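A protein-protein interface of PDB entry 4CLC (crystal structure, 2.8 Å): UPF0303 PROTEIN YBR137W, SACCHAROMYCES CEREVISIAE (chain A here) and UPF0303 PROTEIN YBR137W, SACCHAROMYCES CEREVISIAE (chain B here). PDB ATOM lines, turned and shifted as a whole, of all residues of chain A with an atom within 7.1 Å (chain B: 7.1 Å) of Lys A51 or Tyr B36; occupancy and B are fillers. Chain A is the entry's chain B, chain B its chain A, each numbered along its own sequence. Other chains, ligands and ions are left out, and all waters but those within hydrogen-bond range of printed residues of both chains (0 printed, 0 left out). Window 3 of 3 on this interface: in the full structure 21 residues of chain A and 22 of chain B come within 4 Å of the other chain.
Of the 22 printed residues of chain A, 7 touch a printed residue of chain B.
Printed residues of chain A that touch a printed residue of chain B: Lys A47, Lys A51, Thr A74, Val A75, Thr A76, Tyr A77 and Gly A78.
Hydrophobic or aromatic side chains of chain A within 4 Å of the printed part of chain B: Val A75 and Tyr A77.
Of the 9 printed residues of chain B, 4 touch a printed residue of chain A.
Hydrophobic or aromatic side chains of chain B within 4 Å of the printed part of chain A: Tyr B36, Phe B40 and Leu B71.
Among the printed residues, 10 pairs touch across the chains.
The side-chain amide nitrogen (NE2) of Gln B37 sits at hydrogen-bond distance from the side-chain carboxylate (OD1) of Asp B41 (2.7 Å).
O of Pro A55 is in hydrogen-bond range of NZ of Lys A51, at 3.4 Å.
The side-chain amino group of Lys A51 sits at hydrogen-bond distance from the backbone carbonyl oxygen of Thr A76, 3.1 Å away.
The side-chain hydroxyl of Thr A76 lies within hydrogen-bond range of the backbone carbonyl oxygen of Lys A57 (3.2 Å).
O of Thr A74 sits at hydrogen-bond distance from N of Ile A61 (2.8 Å).
NZ of Lys A47 sits at hydrogen-bond distance from OE1 of Gln B37 (3.4 Å).
Printed residues of chain B within 4 Å of Lys A51: Tyr B36 (3.6 Å).
Tyr B36 touches five residues of chain A.
Of the printed residues of chain A, Leu B71 touches Thr A74 (3.5 Å) and Val A75 (3.7 Å).
Of the printed residues of chain B, Thr A76 touches Tyr B36.
Ile A46 touches none of the printed residues of chain B.
Asn A53 touches none of the printed residues of chain B.
The nearest residue of chain A that does not touch Tyr B36 is Lys A47 (4.9 Å).
The nearest printed residue of chain B that does not touch Tyr A77 is Thr B35 (6.0 Å).
Lys A47 touches Phe B40.
Lys A51 touches Tyr B36 (CE to OH, 3.6 Å).
OG1 of Thr A74 touches CD1 of Phe B40, 3.6 Å away.
Thr A74 touches Leu B71 (CA to O, 3.5 Å).
CD2 of Tyr B36 touches O of Val A75 (3.8 Å).
Val A75 touches Leu B71.
Thr A76 touches Tyr B36 (O to CE2, 3.0 Å).
CA of Tyr A77 touches CG of Tyr B36, at 3.3 Å.
Gly A78 touches Tyr B36 (N to CD1, 3.5 Å).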
ATOM      1  N   TYR A  45     -20.595 -24.875  27.434  1.00  0.00           N
ATOM      2  CA  TYR A  45     -22.037 -24.838  27.633  1.00  0.00           C
ATOM      3  C   TYR A  45     -22.446 -23.875  28.761  1.00  0.00           C
ATOM      4  O   TYR A  45     -23.367 -23.072  28.598  1.00  0.00           O
ATOM      5  CB  TYR A  45     -22.553 -26.253  27.914  1.00  0.00           C
ATOM      6  CG  TYR A  45     -24.030 -26.315  28.210  1.00  0.00           C
ATOM      7  CD1 TYR A  45     -24.969 -26.376  27.183  1.00  0.00           C
ATOM      8  CD2 TYR A  45     -24.493 -26.298  29.517  1.00  0.00           C
ATOM      9  CE1 TYR A  45     -26.325 -26.426  27.453  1.00  0.00           C
ATOM     10  CE2 TYR A  45     -25.849 -26.348  29.799  1.00  0.00           C
ATOM     11  CZ  TYR A  45     -26.759 -26.414  28.765  1.00  0.00           C
ATOM     12  OH  TYR A  45     -28.104 -26.462  29.065  1.00  0.00           O
ATOM     13  N   ILE A  46     -21.739 -23.944  29.888  1.00  0.00           N
ATOM     14  CA  ILE A  46     -22.029 -23.100  31.057  1.00  0.00           C
ATOM     15  C   ILE A  46     -21.595 -21.645  30.852  1.00  0.00           C
ATOM     16  O   ILE A  46     -22.215 -20.723  31.388  1.00  0.00           O
ATOM     17  CB  ILE A  46     -21.336 -23.646  32.327  1.00  0.00           C
ATOM     18  CG1 ILE A  46     -21.673 -25.120  32.532  1.00  0.00           C
ATOM     19  CG2 ILE A  46     -21.729 -22.841  33.551  1.00  0.00           C
ATOM     20  CD1 ILE A  46     -20.777 -25.802  33.519  1.00  0.00           C
ATOM     21  N   LYS A  47     -20.517 -21.443  30.098  1.00  0.00           N
ATOM     22  CA  LYS A  47     -20.101 -20.095  29.746  1.00  0.00           C
ATOM     23  C   LYS A  47     -21.290 -19.404  29.067  1.00  0.00           C
ATOM     24  O   LYS A  47     -21.862 -18.456  29.631  1.00  0.00           O
ATOM     25  CB  LYS A  47     -18.861 -20.101  28.845  1.00  0.00           C
ATOM     26  CG  LYS A  47     -18.092 -18.784  28.876  1.00  0.00           C
ATOM     27  CD  LYS A  47     -17.021 -18.697  27.793  1.00  0.00           C
ATOM     28  CE  LYS A  47     -16.297 -17.372  27.892  1.00  0.00           C
ATOM     29  NZ  LYS A  47     -15.875 -16.794  26.591  1.00  0.00           N
ATOM     30  N   ASN A  48     -21.694 -19.921  27.898  1.00  0.00           N
ATOM     31  CA  ASN A  48     -22.862 -19.411  27.171  1.00  0.00           C
ATOM     32  C   ASN A  48     -24.071 -19.214  28.086  1.00  0.00           C
ATOM     33  O   ASN A  48     -24.719 -18.166  28.074  1.00  0.00           O
ATOM     34  CB  ASN A  48     -23.233 -20.360  26.032  1.00  0.00           C
ATOM     35  CG  ASN A  48     -24.580 -20.006  25.373  1.00  0.00           C
ATOM     36  OD1 ASN A  48     -25.631 -20.603  25.684  1.00  0.00           O
ATOM     37  ND2 ASN A  48     -24.549 -19.032  24.448  1.00  0.00           N
ATOM     38  N   ALA A  49     -24.342 -20.221  28.902  1.00  0.00           N
ATOM     39  CA  ALA A  49     -25.496 -20.199  29.790  1.00  0.00           C
ATOM     40  C   ALA A  49     -25.538 -18.969  30.713  1.00  0.00           C
ATOM     41  O   ALA A  49     -26.556 -18.273  30.768  1.00  0.00           O
ATOM     42  CB  ALA A  49     -25.533 -21.474  30.613  1.00  0.00           C
ATOM     43  N   VAL A  50     -24.454 -18.699  31.439  1.00  0.00           N
ATOM     44  CA  VAL A  50     -24.455 -17.558  32.351  1.00  0.00           C
ATOM     45  C   VAL A  50     -24.382 -16.254  31.547  1.00  0.00           C
ATOM     46  O   VAL A  50     -24.910 -15.221  31.980  1.00  0.00           O
ATOM     47  CB  VAL A  50     -23.287 -17.607  33.401  1.00  0.00           C
ATOM     48  CG1 VAL A  50     -23.454 -18.775  34.348  1.00  0.00           C
ATOM     49  CG2 VAL A  50     -21.930 -17.665  32.730  1.00  0.00           C
ATOM     50  N   LYS A  51     -23.753 -16.301  30.371  1.00  0.00           N
ATOM     51  CA  LYS A  51     -23.686 -15.110  29.527  1.00  0.00           C
ATOM     52  C   LYS A  51     -25.079 -14.698  29.000  1.00  0.00           C
ATOM     53  O   LYS A  51     -25.325 -13.511  28.723  1.00  0.00           O
ATOM     54  CB  LYS A  51     -22.710 -15.326  28.370  1.00  0.00           C
ATOM     55  CG  LYS A  51     -21.259 -15.296  28.812  1.00  0.00           C
ATOM     56  CD  LYS A  51     -20.311 -14.816  27.714  1.00  0.00           C
ATOM     57  CE  LYS A  51     -20.609 -13.381  27.298  1.00  0.00           C
ATOM     58  NZ  LYS A  51     -21.037 -12.516  28.443  1.00  0.00           N
ATOM     59  N   GLU A  52     -25.988 -15.671  28.875  1.00  0.00           N
ATOM     60  CA  GLU A  52     -27.377 -15.363  28.552  1.00  0.00           C
ATOM     61  C   GLU A  52     -28.073 -14.790  29.790  1.00  0.00           C
ATOM     62  O   GLU A  52     -28.392 -13.605  29.824  1.00  0.00           O
ATOM     63  CB  GLU A  52     -28.107 -16.598  28.039  1.00  0.00           C
ATOM     64  N   ASN A  53     -28.269 -15.619  30.810  1.00  0.00           N
ATOM     65  CA  ASN A  53     -28.955 -15.209  32.036  1.00  0.00           C
ATOM     66  C   ASN A  53     -28.366 -13.989  32.742  1.00  0.00           C
ATOM     67  O   ASN A  53     -29.088 -13.047  33.098  1.00  0.00           O
ATOM     68  CB  ASN A  53     -28.985 -16.366  33.026  1.00  0.00           C
ATOM     69  CG  ASN A  53     -29.979 -17.420  32.643  1.00  0.00           C
ATOM     70  OD1 ASN A  53     -31.120 -17.395  33.102  1.00  0.00           O
ATOM     71  ND2 ASN A  53     -29.564 -18.356  31.792  1.00  0.00           N
ATOM     72  N   PHE A  54     -27.057 -14.021  32.966  1.00  0.00           N
ATOM     73  CA  PHE A  54     -26.382 -12.932  33.660  1.00  0.00           C
ATOM     74  C   PHE A  54     -25.366 -12.321  32.709  1.00  0.00           C
ATOM     75  O   PHE A  54     -24.169 -12.643  32.766  1.00  0.00           O
ATOM     76  CB  PHE A  54     -25.714 -13.431  34.931  1.00  0.00           C
ATOM     77  CG  PHE A  54     -26.633 -14.197  35.835  1.00  0.00           C
ATOM     78  CD1 PHE A  54     -26.871 -15.542  35.627  1.00  0.00           C
ATOM     79  CD2 PHE A  54     -27.244 -13.573  36.913  1.00  0.00           C
ATOM     80  CE1 PHE A  54     -27.706 -16.240  36.475  1.00  0.00           C
ATOM     81  CE2 PHE A  54     -28.078 -14.270  37.772  1.00  0.00           C
ATOM     82  CZ  PHE A  54     -28.313 -15.596  37.556  1.00  0.00           C
ATOM     83  N   PRO A  55     -25.856 -11.441  31.820  1.00  0.00           N
ATOM     84  CA  PRO A  55     -25.150 -10.941  30.632  1.00  0.00           C
ATOM     85  C   PRO A  55     -23.911 -10.102  30.934  1.00  0.00           C
ATOM     86  O   PRO A  55     -22.868 -10.268  30.294  1.00  0.00           O
ATOM     87  CB  PRO A  55     -26.211 -10.082  29.936  1.00  0.00           C
ATOM     88  CG  PRO A  55     -27.090  -9.615  31.050  1.00  0.00           C
ATOM     89  CD  PRO A  55     -27.123 -10.725  32.059  1.00  0.00           C
ATOM     90  N   ASP A  56     -24.048  -9.188  31.884  1.00  0.00           N
ATOM     91  CA  ASP A  56     -23.020  -8.197  32.156  1.00  0.00           C
ATOM     92  C   ASP A  56     -22.124  -8.489  33.372  1.00  0.00           C
ATOM     93  O   ASP A  56     -21.186  -7.737  33.637  1.00  0.00           O
ATOM     94  CB  ASP A  56     -23.706  -6.838  32.294  1.00  0.00           C
ATOM     95  CG  ASP A  56     -25.109  -6.949  32.901  1.00  0.00           C
ATOM     96  OD1 ASP A  56     -25.440  -8.001  33.523  1.00  0.00           O
ATOM     97  OD2 ASP A  56     -25.888  -5.977  32.730  1.00  0.00           O
ATOM     98  N   LYS A  57     -22.399  -9.582  34.090  1.00  0.00           N
ATOM     99  CA  LYS A  57     -21.707  -9.878  35.355  1.00  0.00           C
ATOM    100  C   LYS A  57     -20.517 -10.857  35.199  1.00  0.00           C
ATOM    101  O   LYS A  57     -20.655 -11.944  34.622  1.00  0.00           O
ATOM    102  CB  LYS A  57     -22.717 -10.416  36.392  1.00  0.00           C
ATOM    103  N   ILE A  61     -15.785 -19.952  35.631  1.00  0.00           N
ATOM    104  CA  ILE A  61     -16.206 -21.355  35.619  1.00  0.00           C
ATOM    105  C   ILE A  61     -14.998 -22.275  35.600  1.00  0.00           C
ATOM    106  O   ILE A  61     -14.045 -22.055  34.853  1.00  0.00           O
ATOM    107  CB  ILE A  61     -17.117 -21.691  34.403  1.00  0.00           C
ATOM    108  CG1 ILE A  61     -18.385 -20.830  34.405  1.00  0.00           C
ATOM    109  CG2 ILE A  61     -17.516 -23.167  34.418  1.00  0.00           C
ATOM    110  CD1 ILE A  61     -18.372 -19.726  33.397  1.00  0.00           C
ATOM    111  N   THR A  74     -12.721 -20.825  32.655  1.00  0.00           N
ATOM    112  CA  THR A  74     -12.974 -19.598  31.910  1.00  0.00           C
ATOM    113  C   THR A  74     -13.610 -18.488  32.751  1.00  0.00           C
ATOM    114  O   THR A  74     -13.975 -18.688  33.915  1.00  0.00           O
ATOM    115  CB  THR A  74     -13.882 -19.859  30.706  1.00  0.00           C
ATOM    116  OG1 THR A  74     -13.662 -18.842  29.729  1.00  0.00           O
ATOM    117  CG2 THR A  74     -15.346 -19.851  31.132  1.00  0.00           C
ATOM    118  N   VAL A  75     -13.766 -17.324  32.127  1.00  0.00           N
ATOM    119  CA  VAL A  75     -14.427 -16.192  32.751  1.00  0.00           C
ATOM    120  C   VAL A  75     -15.266 -15.445  31.691  1.00  0.00           C
ATOM    121  O   VAL A  75     -14.863 -15.352  30.524  1.00  0.00           O
ATOM    122  CB  VAL A  75     -13.391 -15.262  33.444  1.00  0.00           C
ATOM    123  CG1 VAL A  75     -12.188 -15.017  32.549  1.00  0.00           C
ATOM    124  CG2 VAL A  75     -14.038 -13.967  33.842  1.00  0.00           C
ATOM    125  N   THR A  76     -16.436 -14.942  32.098  1.00  0.00           N
ATOM    126  CA  THR A  76     -17.446 -14.440  31.160  1.00  0.00           C
ATOM    127  C   THR A  76     -17.544 -12.924  30.867  1.00  0.00           C
ATOM    128  O   THR A  76     -18.400 -12.525  30.082  1.00  0.00           O
ATOM    129  CB  THR A  76     -18.832 -14.872  31.628  1.00  0.00           C
ATOM    130  OG1 THR A  76     -19.244 -14.043  32.721  1.00  0.00           O
ATOM    131  CG2 THR A  76     -18.792 -16.317  32.069  1.00  0.00           C
ATOM    132  N   TYR A  77     -16.698 -12.086  31.467  1.00  0.00           N
ATOM    133  CA  TYR A  77     -16.692 -10.640  31.174  1.00  0.00           C
ATOM    134  C   TYR A  77     -15.541 -10.032  31.957  1.00  0.00           C
ATOM    135  O   TYR A  77     -14.983 -10.690  32.833  1.00  0.00           O
ATOM    136  CB  TYR A  77     -18.025  -9.947  31.534  1.00  0.00           C
ATOM    137  CG  TYR A  77     -18.372  -8.727  30.668  1.00  0.00           C
ATOM    138  CD1 TYR A  77     -17.491  -7.657  30.543  1.00  0.00           C
ATOM    139  CD2 TYR A  77     -19.567  -8.658  29.960  1.00  0.00           C
ATOM    140  CE1 TYR A  77     -17.786  -6.551  29.752  1.00  0.00           C
ATOM    141  CE2 TYR A  77     -19.876  -7.554  29.165  1.00  0.00           C
ATOM    142  CZ  TYR A  77     -18.983  -6.501  29.063  1.00  0.00           C
ATOM    143  OH  TYR A  77     -19.275  -5.399  28.273  1.00  0.00           O
ATOM    144  N   GLY A  78     -15.174  -8.795  31.642  1.00  0.00           N
ATOM    145  CA  GLY A  78     -14.128  -8.097  32.361  1.00  0.00           C
ATOM    146  C   GLY A  78     -14.521  -7.874  33.803  1.00  0.00           C
ATOM    147  O   GLY A  78     -15.688  -8.070  34.156  1.00  0.00           O
ATOM    148  N   GLY A  79     -13.557  -7.476  34.637  1.00  0.00           N
ATOM    149  CA  GLY A  79     -13.841  -7.217  36.033  1.00  0.00           C
ATOM    150  C   GLY A  79     -13.893  -8.474  36.883  1.00  0.00           C
ATOM    151  O   GLY A  79     -14.440  -8.477  37.992  1.00  0.00           O
ATOM    152  N   SER A  80     -13.338  -9.559  36.361  1.00  0.00           N
ATOM    153  CA  SER A  80     -13.016 -10.706  37.204  1.00  0.00           C
ATOM    154  C   SER A  80     -11.604 -10.537  37.742  1.00  0.00           C
ATOM    155  O   SER A  80     -10.726 -10.051  37.037  1.00  0.00           O
ATOM    156  CB  SER A  80     -13.124 -12.011  36.436  1.00  0.00           C
ATOM    157  OG  SER A  80     -12.059 -12.132  35.500  1.00  0.00           O
ATOM    158  N   MET A 159     -27.025 -22.266  38.967  1.00  0.00           N
ATOM    159  CA  MET A 159     -26.492 -22.347  37.620  1.00  0.00           C
ATOM    160  C   MET A 159     -25.728 -23.649  37.487  1.00  0.00           C
ATOM    161  O   MET A 159     -25.895 -24.387  36.517  1.00  0.00           O
ATOM    162  CB  MET A 159     -25.597 -21.154  37.300  1.00  0.00           C
ATOM    163  CG  MET A 159     -26.361 -19.950  36.778  1.00  0.00           C
ATOM    164  SD  MET A 159     -27.338 -20.339  35.312  1.00  0.00           S
ATOM    165  CE  MET A 159     -26.059 -21.022  34.254  1.00  0.00           C
ATOM    166  N   PHE B  34      -6.836  -6.552  24.449  1.00  0.00           N
ATOM    167  CA  PHE B  34      -6.827  -7.768  25.246  1.00  0.00           C
ATOM    168  C   PHE B  34      -7.976  -7.680  26.234  1.00  0.00           C
ATOM    169  O   PHE B  34      -7.926  -6.894  27.176  1.00  0.00           O
ATOM    170  CB  PHE B  34      -5.490  -7.925  25.967  1.00  0.00           C
ATOM    171  CG  PHE B  34      -5.343  -9.217  26.714  1.00  0.00           C
ATOM    172  CD1 PHE B  34      -4.872 -10.357  26.072  1.00  0.00           C
ATOM    173  CD2 PHE B  34      -5.654  -9.288  28.059  1.00  0.00           C
ATOM    174  CE1 PHE B  34      -4.721 -11.553  26.755  1.00  0.00           C
ATOM    175  CE2 PHE B  34      -5.503 -10.473  28.753  1.00  0.00           C
ATOM    176  CZ  PHE B  34      -5.036 -11.610  28.100  1.00  0.00           C
ATOM    177  N   THR B  35      -8.995  -8.510  26.039  1.00  0.00           N
ATOM    178  CA  THR B  35     -10.182  -8.493  26.891  1.00  0.00           C
ATOM    179  C   THR B  35     -10.534  -9.898  27.336  1.00  0.00           C
ATOM    180  O   THR B  35      -9.897 -10.863  26.911  1.00  0.00           O
ATOM    181  CB  THR B  35     -11.406  -7.898  26.176  1.00  0.00           C
ATOM    182  OG1 THR B  35     -12.474  -7.747  27.118  1.00  0.00           O
ATOM    183  CG2 THR B  35     -11.884  -8.817  25.062  1.00  0.00           C
ATOM    184  N   TYR B  36     -11.567 -10.012  28.166  1.00  0.00           N
ATOM    185  CA  TYR B  36     -12.021 -11.311  28.625  1.00  0.00           C
ATOM    186  C   TYR B  36     -12.339 -12.192  27.422  1.00  0.00           C
ATOM    187  O   TYR B  36     -12.030 -13.389  27.419  1.00  0.00           O
ATOM    188  CB  TYR B  36     -13.240 -11.171  29.528  1.00  0.00           C
ATOM    189  CG  TYR B  36     -14.543 -11.067  28.773  1.00  0.00           C
ATOM    190  CD1 TYR B  36     -15.020  -9.842  28.334  1.00  0.00           C
ATOM    191  CD2 TYR B  36     -15.299 -12.201  28.497  1.00  0.00           C
ATOM    192  CE1 TYR B  36     -16.222  -9.752  27.642  1.00  0.00           C
ATOM    193  CE2 TYR B  36     -16.491 -12.121  27.801  1.00  0.00           C
ATOM    194  CZ  TYR B  36     -16.953 -10.899  27.379  1.00  0.00           C
ATOM    195  OH  TYR B  36     -18.148 -10.836  26.691  1.00  0.00           O
ATOM    196  N   GLN B  37     -12.936 -11.597  26.388  1.00  0.00           N
ATOM    197  CA  GLN B  37     -13.322 -12.372  25.215  1.00  0.00           C
ATOM    198  C   GLN B  37     -12.132 -12.650  24.305  1.00  0.00           C
ATOM    199  O   GLN B  37     -12.041 -13.734  23.724  1.00  0.00           O
ATOM    200  CB  GLN B  37     -14.427 -11.673  24.432  1.00  0.00           C
ATOM    201  CG  GLN B  37     -14.885 -12.459  23.208  1.00  0.00           C
ATOM    202  CD  GLN B  37     -15.516 -13.803  23.564  1.00  0.00           C
ATOM    203  OE1 GLN B  37     -16.093 -13.971  24.646  1.00  0.00           O
ATOM    204  NE2 GLN B  37     -15.406 -14.767  22.650  1.00  0.00           N
ATOM    205  N   ASP B  38     -11.233 -11.677  24.180  1.00  0.00           N
ATOM    206  CA  ASP B  38      -9.988 -11.878  23.443  1.00  0.00           C
ATOM    207  C   ASP B  38      -9.337 -13.143  23.943  1.00  0.00           C
ATOM    208  O   ASP B  38      -8.914 -13.994  23.163  1.00  0.00           O
ATOM    209  CB  ASP B  38      -9.016 -10.704  23.622  1.00  0.00           C
ATOM    210  CG  ASP B  38      -9.373  -9.494  22.778  1.00  0.00           C
ATOM    211  OD1 ASP B  38      -9.650  -9.654  21.566  1.00  0.00           O
ATOM    212  OD2 ASP B  38      -9.359  -8.376  23.332  1.00  0.00           O
ATOM    213  N   ALA B  39      -9.280 -13.260  25.266  1.00  0.00           N
ATOM    214  CA  ALA B  39      -8.580 -14.356  25.909  1.00  0.00           C
ATOM    215  C   ALA B  39      -9.214 -15.685  25.533  1.00  0.00           C
ATOM    216  O   ALA B  39      -8.522 -16.651  25.210  1.00  0.00           O
ATOM    217  CB  ALA B  39      -8.578 -14.166  27.408  1.00  0.00           C
ATOM    218  N   PHE B  40     -10.537 -15.726  25.570  1.00  0.00           N
ATOM    219  CA  PHE B  40     -11.238 -16.925  25.149  1.00  0.00           C
ATOM    220  C   PHE B  40     -10.906 -17.216  23.694  1.00  0.00           C
ATOM    221  O   PHE B  40     -10.480 -18.325  23.360  1.00  0.00           O
ATOM    222  CB  PHE B  40     -12.745 -16.775  25.334  1.00  0.00           C
ATOM    223  CG  PHE B  40     -13.509 -18.040  25.087  1.00  0.00           C
ATOM    224  CD1 PHE B  40     -13.674 -18.974  26.096  1.00  0.00           C
ATOM    225  CD2 PHE B  40     -14.069 -18.300  23.844  1.00  0.00           C
ATOM    226  CE1 PHE B  40     -14.388 -20.141  25.873  1.00  0.00           C
ATOM    227  CE2 PHE B  40     -14.778 -19.467  23.615  1.00  0.00           C
ATOM    228  CZ  PHE B  40     -14.938 -20.388  24.631  1.00  0.00           C
ATOM    229  N   ASP B  41     -11.089 -16.204  22.841  1.00  0.00           N
ATOM    230  CA  ASP B  41     -10.816 -16.337  21.413  1.00  0.00           C
ATOM    231  C   ASP B  41      -9.413 -16.891  21.214  1.00  0.00           C
ATOM    232  O   ASP B  41      -9.226 -17.857  20.474  1.00  0.00           O
ATOM    233  CB  ASP B  41     -10.971 -14.995  20.673  1.00  0.00           C
ATOM    234  CG  ASP B  41     -12.418 -14.478  20.659  1.00  0.00           C
ATOM    235  OD1 ASP B  41     -13.356 -15.276  20.911  1.00  0.00           O
ATOM    236  OD2 ASP B  41     -12.619 -13.268  20.376  1.00  0.00           O
ATOM    237  N   LEU B  71      -7.427 -16.565  33.248  1.00  0.00           N
ATOM    238  CA  LEU B  71      -8.496 -16.321  32.275  1.00  0.00           C
ATOM    239  C   LEU B  71      -8.929 -17.542  31.446  1.00  0.00           C
ATOM    240  O   LEU B  71     -10.125 -17.750  31.201  1.00  0.00           O
ATOM    241  CB  LEU B  71      -8.063 -15.218  31.326  1.00  0.00           C
ATOM    242  CG  LEU B  71      -7.631 -13.934  32.024  1.00  0.00           C
ATOM    243  CD1 LEU B  71      -7.013 -13.020  30.991  1.00  0.00           C
ATOM    244  CD2 LEU B  71      -8.808 -13.264  32.716  1.00  0.00           C
